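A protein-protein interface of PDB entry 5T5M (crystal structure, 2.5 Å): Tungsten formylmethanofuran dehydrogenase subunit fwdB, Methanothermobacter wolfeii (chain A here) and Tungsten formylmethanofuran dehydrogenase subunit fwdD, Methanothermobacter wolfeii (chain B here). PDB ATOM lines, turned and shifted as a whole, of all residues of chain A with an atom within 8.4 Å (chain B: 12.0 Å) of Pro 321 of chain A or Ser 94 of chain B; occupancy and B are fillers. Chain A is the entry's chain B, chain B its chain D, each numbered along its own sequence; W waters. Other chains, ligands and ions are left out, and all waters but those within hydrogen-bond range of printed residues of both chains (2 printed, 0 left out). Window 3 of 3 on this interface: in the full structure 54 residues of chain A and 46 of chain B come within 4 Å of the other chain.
OD2 of Asp 328 of chain A is in hydrogen-bond range of N of Gly 325 of chain A. NH2 of Arg 89 of chain B is in salt-bridge range of OD1 of Asp 93 of chain B. OG of Ser 99 of chain B sits at hydrogen-bond distance from NH1 of Arg 89 of chain B (2.9 Å). OG1 of Thr 92 of chain B lies close to N of Ser 94 of chain B (3.4 Å). The side-chain hydroxyl (OG1) of Thr 92 of chain B sits at hydrogen-bond distance from the backbone NH (N) of Ala 96 of chain B (3.3 Å). The side-chain hydroxyl (OG1) of Thr 95 of chain B sits at hydrogen-bond distance from the backbone NH (N) of Thr 97 of chain B (3.1 Å).
Water W2 lies within hydrogen-bond range of OG of Ser 116 of chain A (2.6 Å) and O of Ala 96 of chain B (2.7 Å). Water W1 lies within hydrogen-bond range of the side-chain hydroxyl of Tyr 308 of chain A (2.8 Å), the side-chain hydroxyl of Thr 97 of chain B (2.8 Å) and the backbone carbonyl oxygen of Thr 95 of chain B (2.8 Å).
Of the printed residues of chain B, Ser 116 of chain A touches Ala 96 (2.9 Å) and Thr 97 (2.9 Å). No residue of chain B comes within 4 Å of Tyr 308 of chain A. No residue of chain B comes within 4 Å of Cys 309 of chain A. No residue of chain B comes within 4 Å of Tyr 319 of chain A. No residue of chain B comes within 4 Å of Asn 320 of chain A. Of the printed residues of chain B, Pro 321 of chain A touches Ser 94 and Thr 95. Of chain B, only Ser 94 (3.3 Å), Thr 95 (3.7 Å) and Ala 96 (3.7 Å) come within 4 Å of Gly 322 of chain A. No residue of chain B comes within 4 Å of Thr 324 of chain A. Gly 325 of chain A touches just one residue of chain B: Ala 96. Pro 90 of chain B touches none of the printed residues of chain A. Of chain A, only Leu 124 (3.96 Å), Lys 262 (3.8 Å), His 263 (3.6 Å), Pro 321 (3.9 Å) and Gly 322 (3.7 Å) come within 4 Å of Thr 95 of chain B. Of the printed residues of chain A, Ala 96 of chain B touches Ser 116, Gly 322, Gly 325 and Asp 328. Of the printed residues of chain A, Thr 97 of chain B touches Ser 116, Pro 121 and Lys 262. The nearest residue of chain B that does not touch Pro 321 of chain A is Ala 96 of chain B (4.5 Å). The nearest printed residue of chain B that does not touch Pro 121 of chain A is Thr 95 of chain B (5.2 Å).
Thr 97 of chain B touches Pro 121 of chain A. O of Thr 95 of chain B touches CD1 of Leu 124 of chain A (3.96 Å). Lys 262 of chain A touches Thr 95 of chain B (CD to OG1, 3.8 Å). Thr 95 of chain B touches His 263 of chain A (CG2 to ND1, 3.6 Å). Pro 321 of chain A touches Thr 95 of chain B. C of Ser 94 of chain B touches CA of Gly 322 of chain A (3.3 Å). N of Gly 322 of chain A touches C of Thr 95 of chain B, 3.7 Å away. Gly 322 of chain A touches Ala 96 of chain B. Gly 325 of chain A touches Ala 96 of chain B (CA to CB, 3.9 Å). Asp 328 of chain A touches Ala 96 of chain B.
Of the 11 printed residues of chain B, 9 touch a printed residue of chain A. Hydrophobic or aromatic side chains of chain B within 4 Å of the printed part of chain A: Ala 96. Printed residues of chain A that touch a printed residue of chain B: Ser 116, Pro 121, Leu 124, Lys 262, His 263, Pro 321, Gly 322, Gly 325 and Asp 328. Among the printed residues, 20 pairs touch across the chains.
O of Ser 116 of chain A sits at hydrogen-bond distance from OG1 of Thr 97 of chain B. The backbone carbonyl oxygen (O) of Tyr 91 of chain B is in hydrogen-bond range of the side-chain amino group (NZ) of Lys 262 of chain A (3.3 Å). NZ of Lys 262 of chain A lies within hydrogen-bond range of O of Thr 92 of chain B (3.5 Å). OD2 of Asp 93 of chain B is in salt-bridge range of NZ of Lys 262 of chain A (2.7 Å). The side-chain amino group of Lys 262 of chain A is in hydrogen-bond range of the backbone carbonyl oxygen of Thr 97 of chain B (2.8 Å). The side-chain hydroxyl (OG) of Ser 99 of chain B lies within hydrogen-bond range of the side-chain amino group (NZ) of Lys 262 of chain A, 3.0 Å away. The side-chain carboxylate (OD1) of Asp 328 of chain A is in hydrogen-bond range of the side-chain hydroxyl (OG1) of Thr 92 of chain B (3.1 Å). The backbone carbonyl oxygen (O) of Ser 116 of chain A sits close to the backbone carbonyl oxygen (O) of Ala 96 of chain B (2.9 Å). O of Pro 321 of chain A sits close to O of Ser 94 of chain B, at 3.3 Å.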
ATOM      1  N   ASP A 112       1.715  24.552  30.204  1.00  0.00           N
ATOM      2  CA  ASP A 112       2.818  25.479  30.035  1.00  0.00           C
ATOM      3  C   ASP A 112       2.581  26.699  30.919  1.00  0.00           C
ATOM      4  O   ASP A 112       1.437  27.118  31.121  1.00  0.00           O
ATOM      5  CB  ASP A 112       2.950  25.885  28.560  1.00  0.00           C
ATOM      6  CG  ASP A 112       4.150  26.753  28.306  1.00  0.00           C
ATOM      7  OD1 ASP A 112       5.184  26.520  28.958  1.00  0.00           O
ATOM      8  OD2 ASP A 112       4.064  27.666  27.461  1.00  0.00           O
ATOM      9  N   SER A 116       7.637  30.288  29.165  1.00  0.00           N
ATOM     10  CA  SER A 116       7.784  30.216  27.715  1.00  0.00           C
ATOM     11  C   SER A 116       7.708  31.581  27.043  1.00  0.00           C
ATOM     12  O   SER A 116       7.913  31.656  25.831  1.00  0.00           O
ATOM     13  CB  SER A 116       6.729  29.275  27.105  1.00  0.00           C
ATOM     14  OG  SER A 116       5.423  29.835  27.069  1.00  0.00           O
ATOM     15  N   GLY A 120      12.119  30.800  30.010  1.00  0.00           N
ATOM     16  CA  GLY A 120      12.206  29.592  29.231  1.00  0.00           C
ATOM     17  C   GLY A 120      13.509  29.501  28.452  1.00  0.00           C
ATOM     18  O   GLY A 120      14.172  28.464  28.441  1.00  0.00           O
ATOM     19  N   PRO A 121      13.904  30.584  27.772  1.00  0.00           N
ATOM     20  CA  PRO A 121      15.235  30.570  27.142  1.00  0.00           C
ATOM     21  C   PRO A 121      16.345  30.263  28.132  1.00  0.00           C
ATOM     22  O   PRO A 121      17.321  29.591  27.775  1.00  0.00           O
ATOM     23  CB  PRO A 121      15.356  31.984  26.546  1.00  0.00           C
ATOM     24  CG  PRO A 121      13.955  32.381  26.253  1.00  0.00           C
ATOM     25  CD  PRO A 121      13.136  31.789  27.398  1.00  0.00           C
ATOM     26  N   VAL A 123      15.896  28.368  30.724  1.00  0.00           N
ATOM     27  CA  VAL A 123      15.703  26.951  31.010  1.00  0.00           C
ATOM     28  C   VAL A 123      16.356  26.106  29.923  1.00  0.00           C
ATOM     29  O   VAL A 123      17.045  25.121  30.210  1.00  0.00           O
ATOM     30  CB  VAL A 123      14.201  26.645  31.156  1.00  0.00           C
ATOM     31  CG1 VAL A 123      13.949  25.141  31.282  1.00  0.00           C
ATOM     32  CG2 VAL A 123      13.619  27.397  32.367  1.00  0.00           C
ATOM     33  N   LEU A 124      16.144  26.478  28.656  1.00  0.00           N
ATOM     34  CA  LEU A 124      16.798  25.794  27.543  1.00  0.00           C
ATOM     35  C   LEU A 124      18.318  25.908  27.632  1.00  0.00           C
ATOM     36  O   LEU A 124      19.038  24.939  27.363  1.00  0.00           O
ATOM     37  CB  LEU A 124      16.303  26.376  26.226  1.00  0.00           C
ATOM     38  CG  LEU A 124      14.821  26.185  25.920  1.00  0.00           C
ATOM     39  CD1 LEU A 124      14.387  27.098  24.774  1.00  0.00           C
ATOM     40  CD2 LEU A 124      14.584  24.735  25.579  1.00  0.00           C
ATOM     41  N   GLN A 127      19.645  23.623  30.490  1.00  0.00           N
ATOM     42  CA  GLN A 127      19.598  22.212  30.116  1.00  0.00           C
ATOM     43  C   GLN A 127      20.796  21.814  29.255  1.00  0.00           C
ATOM     44  O   GLN A 127      21.222  20.653  29.286  1.00  0.00           O
ATOM     45  CB  GLN A 127      18.291  21.916  29.382  1.00  0.00           C
ATOM     46  CG  GLN A 127      17.078  21.988  30.283  1.00  0.00           C
ATOM     47  CD  GLN A 127      15.766  21.935  29.533  1.00  0.00           C
ATOM     48  OE1 GLN A 127      15.686  22.289  28.352  1.00  0.00           O
ATOM     49  NE2 GLN A 127      14.721  21.485  30.219  1.00  0.00           N
ATOM     50  N   LYS A 262      18.151  34.701  21.968  1.00  0.00           N
ATOM     51  CA  LYS A 262      17.344  34.164  23.058  1.00  0.00           C
ATOM     52  C   LYS A 262      18.138  33.199  23.934  1.00  0.00           C
ATOM     53  O   LYS A 262      19.066  33.628  24.629  1.00  0.00           O
ATOM     54  CB  LYS A 262      16.093  33.521  22.471  1.00  0.00           C
ATOM     55  CG  LYS A 262      15.245  34.580  21.761  1.00  0.00           C
ATOM     56  CD  LYS A 262      14.075  34.031  20.982  1.00  0.00           C
ATOM     57  CE  LYS A 262      13.267  35.179  20.387  1.00  0.00           C
ATOM     58  NZ  LYS A 262      12.261  34.719  19.405  1.00  0.00           N
ATOM     59  N   HIS A 263      17.798  31.905  23.915  1.00  0.00           N
ATOM     60  CA  HIS A 263      18.429  30.969  24.845  1.00  0.00           C
ATOM     61  C   HIS A 263      19.942  30.923  24.671  1.00  0.00           C
ATOM     62  O   HIS A 263      20.663  30.601  25.622  1.00  0.00           O
ATOM     63  CB  HIS A 263      17.839  29.568  24.677  1.00  0.00           C
ATOM     64  CG  HIS A 263      18.027  28.997  23.313  1.00  0.00           C
ATOM     65  ND1 HIS A 263      17.478  29.570  22.184  1.00  0.00           N
ATOM     66  CD2 HIS A 263      18.721  27.917  22.889  1.00  0.00           C
ATOM     67  CE1 HIS A 263      17.821  28.863  21.125  1.00  0.00           C
ATOM     68  NE2 HIS A 263      18.578  27.855  21.525  1.00  0.00           N
ATOM     69  N   TYR A 306       9.808  17.093  33.383  1.00  0.00           N
ATOM     70  CA  TYR A 306      10.065  18.230  32.507  1.00  0.00           C
ATOM     71  C   TYR A 306       9.499  19.521  33.106  1.00  0.00           C
ATOM     72  O   TYR A 306       8.480  19.488  33.812  1.00  0.00           O
ATOM     73  CB  TYR A 306       9.446  18.031  31.120  1.00  0.00           C
ATOM     74  CG  TYR A 306      10.014  16.889  30.311  1.00  0.00           C
ATOM     75  CD1 TYR A 306      11.292  16.961  29.781  1.00  0.00           C
ATOM     76  CD2 TYR A 306       9.251  15.758  30.035  1.00  0.00           C
ATOM     77  CE1 TYR A 306      11.809  15.938  29.025  1.00  0.00           C
ATOM     78  CE2 TYR A 306       9.760  14.727  29.272  1.00  0.00           C
ATOM     79  CZ  TYR A 306      11.042  14.824  28.771  1.00  0.00           C
ATOM     80  OH  TYR A 306      11.564  13.804  28.016  1.00  0.00           O
ATOM     81  N   PRO A 307      10.105  20.684  32.791  1.00  0.00           N
ATOM     82  CA  PRO A 307       9.762  21.933  33.501  1.00  0.00           C
ATOM     83  C   PRO A 307       8.607  22.760  32.938  1.00  0.00           C
ATOM     84  O   PRO A 307       7.945  23.469  33.703  1.00  0.00           O
ATOM     85  CB  PRO A 307      11.066  22.733  33.417  1.00  0.00           C
ATOM     86  CG  PRO A 307      11.707  22.251  32.149  1.00  0.00           C
ATOM     87  CD  PRO A 307      11.356  20.807  32.023  1.00  0.00           C
ATOM     88  N   TYR A 308       8.393  22.731  31.625  1.00  0.00           N
ATOM     89  CA  TYR A 308       7.344  23.518  30.973  1.00  0.00           C
ATOM     90  C   TYR A 308       7.247  23.026  29.532  1.00  0.00           C
ATOM     91  O   TYR A 308       8.037  22.191  29.095  1.00  0.00           O
ATOM     92  CB  TYR A 308       7.629  25.038  31.057  1.00  0.00           C
ATOM     93  CG  TYR A 308       8.686  25.565  30.091  1.00  0.00           C
ATOM     94  CD1 TYR A 308       9.889  24.885  29.884  1.00  0.00           C
ATOM     95  CD2 TYR A 308       8.479  26.747  29.385  1.00  0.00           C
ATOM     96  CE1 TYR A 308      10.851  25.371  28.993  1.00  0.00           C
ATOM     97  CE2 TYR A 308       9.427  27.227  28.488  1.00  0.00           C
ATOM     98  CZ  TYR A 308      10.609  26.539  28.295  1.00  0.00           C
ATOM     99  OH  TYR A 308      11.543  27.034  27.406  1.00  0.00           O
ATOM    100  N   CYS A 309       6.264  23.538  28.797  1.00  0.00           N
ATOM    101  CA  CYS A 309       5.955  23.012  27.459  1.00  0.00           C
ATOM    102  C   CYS A 309       5.802  21.491  27.498  1.00  0.00           C
ATOM    103  O   CYS A 309       6.391  20.770  26.703  1.00  0.00           O
ATOM    104  CB  CYS A 309       7.041  23.385  26.443  1.00  0.00           C
ATOM    105  SG  CYS A 309       7.505  25.112  26.286  1.00  0.00           S
ATOM    106  N   VAL A 310       5.026  20.984  28.448  1.00  0.00           N
ATOM    107  CA  VAL A 310       4.893  19.542  28.635  1.00  0.00           C
ATOM    108  C   VAL A 310       3.629  19.070  27.943  1.00  0.00           C
ATOM    109  O   VAL A 310       2.535  19.574  28.216  1.00  0.00           O
ATOM    110  CB  VAL A 310       4.872  19.174  30.125  1.00  0.00           C
ATOM    111  CG1 VAL A 310       4.748  17.663  30.301  1.00  0.00           C
ATOM    112  CG2 VAL A 310       6.128  19.684  30.791  1.00  0.00           C
ATOM    113  N   ARG A 318       6.143  14.375  27.185  1.00  0.00           N
ATOM    114  CA  ARG A 318       7.056  14.710  26.103  1.00  0.00           C
ATOM    115  C   ARG A 318       7.252  16.217  26.085  1.00  0.00           C
ATOM    116  O   ARG A 318       6.393  16.975  26.544  1.00  0.00           O
ATOM    117  CB  ARG A 318       6.546  14.206  24.756  1.00  0.00           C
ATOM    118  CG  ARG A 318       6.556  12.686  24.653  1.00  0.00           C
ATOM    119  CD  ARG A 318       6.098  12.223  23.307  1.00  0.00           C
ATOM    120  NE  ARG A 318       4.804  12.804  22.962  1.00  0.00           N
ATOM    121  CZ  ARG A 318       4.374  12.987  21.717  1.00  0.00           C
ATOM    122  NH1 ARG A 318       5.134  12.637  20.683  1.00  0.00           N
ATOM    123  NH2 ARG A 318       3.182  13.527  21.507  1.00  0.00           N
ATOM    124  N   TYR A 319       8.404  16.642  25.569  1.00  0.00           N
ATOM    125  CA  TYR A 319       8.892  17.994  25.808  1.00  0.00           C
ATOM    126  C   TYR A 319       9.669  18.490  24.596  1.00  0.00           C
ATOM    127  O   TYR A 319      10.677  17.887  24.211  1.00  0.00           O
ATOM    128  CB  TYR A 319       9.760  17.993  27.074  1.00  0.00           C
ATOM    129  CG  TYR A 319      10.585  19.234  27.338  1.00  0.00           C
ATOM    130  CD1 TYR A 319      10.005  20.372  27.872  1.00  0.00           C
ATOM    131  CD2 TYR A 319      11.956  19.254  27.089  1.00  0.00           C
ATOM    132  CE1 TYR A 319      10.754  21.503  28.134  1.00  0.00           C
ATOM    133  CE2 TYR A 319      12.717  20.380  27.354  1.00  0.00           C
ATOM    134  CZ  TYR A 319      12.105  21.503  27.877  1.00  0.00           C
ATOM    135  OH  TYR A 319      12.823  22.641  28.155  1.00  0.00           O
ATOM    136  N   ASN A 320       9.208  19.591  24.002  1.00  0.00           N
ATOM    137  CA  ASN A 320       9.870  20.175  22.837  1.00  0.00           C
ATOM    138  C   ASN A 320       9.554  21.662  22.727  1.00  0.00           C
ATOM    139  O   ASN A 320       8.786  22.061  21.849  1.00  0.00           O
ATOM    140  CB  ASN A 320       9.434  19.475  21.546  1.00  0.00           C
ATOM    141  CG  ASN A 320       9.825  18.004  21.498  1.00  0.00           C
ATOM    142  OD1 ASN A 320      10.893  17.647  20.989  1.00  0.00           O
ATOM    143  ND2 ASN A 320       8.945  17.137  22.005  1.00  0.00           N
ATOM    144  N   PRO A 321      10.120  22.514  23.577  1.00  0.00           N
ATOM    145  CA  PRO A 321       9.939  23.958  23.384  1.00  0.00           C
ATOM    146  C   PRO A 321      10.277  24.356  21.950  1.00  0.00           C
ATOM    147  O   PRO A 321      11.299  23.943  21.394  1.00  0.00           O
ATOM    148  CB  PRO A 321      10.904  24.575  24.403  1.00  0.00           C
ATOM    149  CG  PRO A 321      11.053  23.542  25.448  1.00  0.00           C
ATOM    150  CD  PRO A 321      10.982  22.220  24.737  1.00  0.00           C
ATOM    151  N   GLY A 322       9.400  25.162  21.351  1.00  0.00           N
ATOM    152  CA  GLY A 322       9.383  25.411  19.920  1.00  0.00           C
ATOM    153  C   GLY A 322       8.250  24.694  19.214  1.00  0.00           C
ATOM    154  O   GLY A 322       7.820  25.133  18.137  1.00  0.00           O
ATOM    155  N   GLU A 323       7.769  23.595  19.797  1.00  0.00           N
ATOM    156  CA  GLU A 323       6.556  22.898  19.383  1.00  0.00           C
ATOM    157  C   GLU A 323       5.478  22.954  20.452  1.00  0.00           C
ATOM    158  O   GLU A 323       4.354  23.388  20.175  1.00  0.00           O
ATOM    159  CB  GLU A 323       6.873  21.424  19.055  1.00  0.00           C
ATOM    160  CG  GLU A 323       5.641  20.573  18.741  1.00  0.00           C
ATOM    161  CD  GLU A 323       5.937  19.085  18.729  1.00  0.00           C
ATOM    162  OE1 GLU A 323       6.885  18.667  19.422  1.00  0.00           O
ATOM    163  OE2 GLU A 323       5.209  18.333  18.044  1.00  0.00           O
ATOM    164  N   THR A 324       5.792  22.528  21.673  1.00  0.00           N
ATOM    165  CA  THR A 324       4.801  22.343  22.720  1.00  0.00           C
ATOM    166  C   THR A 324       4.711  23.544  23.653  1.00  0.00           C
ATOM    167  O   THR A 324       4.178  23.419  24.759  1.00  0.00           O
ATOM    168  CB  THR A 324       5.116  21.070  23.512  1.00  0.00           C
ATOM    169  OG1 THR A 324       6.374  21.210  24.190  1.00  0.00           O
ATOM    170  CG2 THR A 324       5.212  19.875  22.567  1.00  0.00           C
ATOM    171  N   GLY A 325       5.231  24.701  23.232  1.00  0.00           N
ATOM    172  CA  GLY A 325       5.027  25.922  23.979  1.00  0.00           C
ATOM    173  C   GLY A 325       3.705  26.592  23.645  1.00  0.00           C
ATOM    174  O   GLY A 325       3.104  26.356  22.592  1.00  0.00           O
ATOM    175  N   ALA A 326       3.260  27.458  24.561  1.00  0.00           N
ATOM    176  CA  ALA A 326       1.962  28.117  24.401  1.00  0.00           C
ATOM    177  C   ALA A 326       1.894  28.908  23.096  1.00  0.00           C
ATOM    178  O   ALA A 326       0.927  28.788  22.335  1.00  0.00           O
ATOM    179  CB  ALA A 326       1.682  29.025  25.598  1.00  0.00           C
ATOM    180  N   ASP A 328       3.662  28.541  20.448  1.00  0.00           N
ATOM    181  CA  ASP A 328       3.779  27.652  19.297  1.00  0.00           C
ATOM    182  C   ASP A 328       2.430  27.041  18.930  1.00  0.00           C
ATOM    183  O   ASP A 328       2.035  27.047  17.760  1.00  0.00           O
ATOM    184  CB  ASP A 328       4.801  26.556  19.593  1.00  0.00           C
ATOM    185  CG  ASP A 328       6.117  27.107  20.104  1.00  0.00           C
ATOM    186  OD1 ASP A 328       6.686  28.012  19.443  1.00  0.00           O
ATOM    187  OD2 ASP A 328       6.580  26.633  21.170  1.00  0.00           O
ATOM    188  N   ASN A 332       0.799  28.351  15.379  1.00  0.00           N
ATOM    189  CA  ASN A 332       0.656  27.312  14.378  1.00  0.00           C
ATOM    190  C   ASN A 332      -0.761  26.753  14.341  1.00  0.00           C
ATOM    191  O   ASN A 332      -1.042  25.834  13.561  1.00  0.00           O
ATOM    192  CB  ASN A 332       1.684  26.215  14.654  1.00  0.00           C
ATOM    193  CG  ASN A 332       3.105  26.755  14.643  1.00  0.00           C
ATOM    194  OD1 ASN A 332       3.423  27.647  13.858  1.00  0.00           O
ATOM    195  ND2 ASN A 332       3.954  26.245  15.538  1.00  0.00           N
ATOM    196  N   ARG B  89       7.557  41.359  17.155  1.00  0.00           N
ATOM    197  CA  ARG B  89       7.706  40.182  16.303  1.00  0.00           C
ATOM    198  C   ARG B  89       7.181  38.939  17.020  1.00  0.00           C
ATOM    199  O   ARG B  89       7.661  38.621  18.112  1.00  0.00           O
ATOM    200  CB  ARG B  89       9.170  40.000  15.906  1.00  0.00           C
ATOM    201  CG  ARG B  89       9.449  38.739  15.095  1.00  0.00           C
ATOM    202  CD  ARG B  89      10.872  38.701  14.594  1.00  0.00           C
ATOM    203  NE  ARG B  89      11.182  37.461  13.875  1.00  0.00           N
ATOM    204  CZ  ARG B  89      11.787  36.396  14.405  1.00  0.00           C
ATOM    205  NH1 ARG B  89      12.154  36.386  15.673  1.00  0.00           N
ATOM    206  NH2 ARG B  89      12.024  35.329  13.659  1.00  0.00           N
ATOM    207  N   PRO B  90       6.208  38.220  16.453  1.00  0.00           N
ATOM    208  CA  PRO B  90       5.619  37.065  17.152  1.00  0.00           C
ATOM    209  C   PRO B  90       6.465  35.797  17.134  1.00  0.00           C
ATOM    210  O   PRO B  90       6.428  35.005  18.086  1.00  0.00           O
ATOM    211  CB  PRO B  90       4.316  36.834  16.381  1.00  0.00           C
ATOM    212  CG  PRO B  90       4.626  37.330  15.005  1.00  0.00           C
ATOM    213  CD  PRO B  90       5.499  38.526  15.201  1.00  0.00           C
ATOM    214  N   TYR B  91       7.222  35.592  16.060  1.00  0.00           N
ATOM    215  CA  TYR B  91       7.905  34.322  15.834  1.00  0.00           C
ATOM    216  C   TYR B  91       8.897  34.010  16.946  1.00  0.00           C
ATOM    217  O   TYR B  91       9.551  34.904  17.490  1.00  0.00           O
ATOM    218  CB  TYR B  91       8.626  34.359  14.487  1.00  0.00           C
ATOM    219  CG  TYR B  91       7.652  34.539  13.354  1.00  0.00           C
ATOM    220  CD1 TYR B  91       6.798  33.514  12.995  1.00  0.00           C
ATOM    221  CD2 TYR B  91       7.564  35.747  12.666  1.00  0.00           C
ATOM    222  CE1 TYR B  91       5.885  33.673  11.972  1.00  0.00           C
ATOM    223  CE2 TYR B  91       6.661  35.920  11.634  1.00  0.00           C
ATOM    224  CZ  TYR B  91       5.821  34.879  11.293  1.00  0.00           C
ATOM    225  OH  TYR B  91       4.913  35.037  10.276  1.00  0.00           O
ATOM    226  N   THR B  92       9.015  32.722  17.271  1.00  0.00           N
ATOM    227  CA  THR B  92       9.781  32.278  18.427  1.00  0.00           C
ATOM    228  C   THR B  92      11.092  31.615  18.040  1.00  0.00           C
ATOM    229  O   THR B  92      11.884  31.281  18.928  1.00  0.00           O
ATOM    230  CB  THR B  92       8.952  31.308  19.283  1.00  0.00           C
ATOM    231  OG1 THR B  92       8.824  30.053  18.613  1.00  0.00           O
ATOM    232  CG2 THR B  92       7.557  31.865  19.554  1.00  0.00           C
ATOM    233  N   ASP B  93      11.346  31.412  16.745  1.00  0.00           N
ATOM    234  CA  ASP B  93      12.556  30.731  16.298  1.00  0.00           C
ATOM    235  C   ASP B  93      12.670  29.350  16.945  1.00  0.00           C
ATOM    236  O   ASP B  93      13.753  28.896  17.320  1.00  0.00           O
ATOM    237  CB  ASP B  93      13.794  31.584  16.591  1.00  0.00           C
ATOM    238  CG  ASP B  93      13.615  33.027  16.179  1.00  0.00           C
ATOM    239  OD1 ASP B  93      13.887  33.340  15.013  1.00  0.00           O
ATOM    240  OD2 ASP B  93      13.212  33.857  17.013  1.00  0.00           O
ATOM    241  N   SER B  94      11.524  28.691  17.104  1.00  0.00           N
ATOM    242  CA  SER B  94      11.450  27.337  17.657  1.00  0.00           C
ATOM    243  C   SER B  94      11.987  27.271  19.082  1.00  0.00           C
ATOM    244  O   SER B  94      12.609  26.284  19.473  1.00  0.00           O
ATOM    245  CB  SER B  94      12.181  26.338  16.768  1.00  0.00           C
ATOM    246  OG  SER B  94      11.635  26.297  15.455  1.00  0.00           O
ATOM    247  N   THR B  95      11.741  28.334  19.868  1.00  0.00           N
ATOM    248  CA  THR B  95      12.026  28.340  21.297  1.00  0.00           C
ATOM    249  C   THR B  95      10.784  28.495  22.164  1.00  0.00           C
ATOM    250  O   THR B  95      10.878  28.298  23.381  1.00  0.00           O
ATOM    251  CB  THR B  95      12.995  29.474  21.669  1.00  0.00           C
ATOM    252  OG1 THR B  95      12.307  30.733  21.644  1.00  0.00           O
ATOM    253  CG2 THR B  95      14.189  29.513  20.723  1.00  0.00           C
ATOM    254  N   ALA B  96       9.634  28.842  21.586  1.00  0.00           N
ATOM    255  CA  ALA B  96       8.385  29.161  22.269  1.00  0.00           C
ATOM    256  C   ALA B  96       8.337  30.622  22.716  1.00  0.00           C
ATOM    257  O   ALA B  96       7.266  31.091  23.102  1.00  0.00           O
ATOM    258  CB  ALA B  96       8.104  28.267  23.497  1.00  0.00           C
ATOM    259  N   THR B  97       9.448  31.363  22.659  1.00  0.00           N
ATOM    260  CA  THR B  97       9.499  32.714  23.195  1.00  0.00           C
ATOM    261  C   THR B  97       9.462  33.737  22.069  1.00  0.00           C
ATOM    262  O   THR B  97      10.398  33.782  21.253  1.00  0.00           O
ATOM    263  CB  THR B  97      10.752  32.897  24.041  1.00  0.00           C
ATOM    264  OG1 THR B  97      10.720  31.965  25.131  1.00  0.00           O
ATOM    265  CG2 THR B  97      10.808  34.312  24.605  1.00  0.00           C
ATOM    266  N   PRO B  98       8.430  34.567  21.987  1.00  0.00           N
ATOM    267  CA  PRO B  98       8.379  35.594  20.939  1.00  0.00           C
ATOM    268  C   PRO B  98       9.464  36.650  21.109  1.00  0.00           C
ATOM    269  O   PRO B  98       9.995  36.867  22.199  1.00  0.00           O
ATOM    270  CB  PRO B  98       6.986  36.213  21.123  1.00  0.00           C
ATOM    271  CG  PRO B  98       6.215  35.207  21.916  1.00  0.00           C
ATOM    272  CD  PRO B  98       7.196  34.534  22.785  1.00  0.00           C
ATOM    273  N   SER B  99       9.757  37.345  20.010  1.00  0.00           N
ATOM    274  CA  SER B  99      10.724  38.444  20.013  1.00  0.00           C
ATOM    275  C   SER B  99      10.051  39.744  20.454  1.00  0.00           C
ATOM    276  O   SER B  99       9.639  40.563  19.636  1.00  0.00           O
ATOM    277  CB  SER B  99      11.349  38.600  18.638  1.00  0.00           C
ATOM    278  OG  SER B  99      12.231  37.535  18.364  1.00  0.00           O
HETATM  279  O   HOH W   1      11.257  29.368  25.950  1.00  0.00           O
HETATM  280  O   HOH W   2       5.048  30.666  24.604  1.00  0.00           O
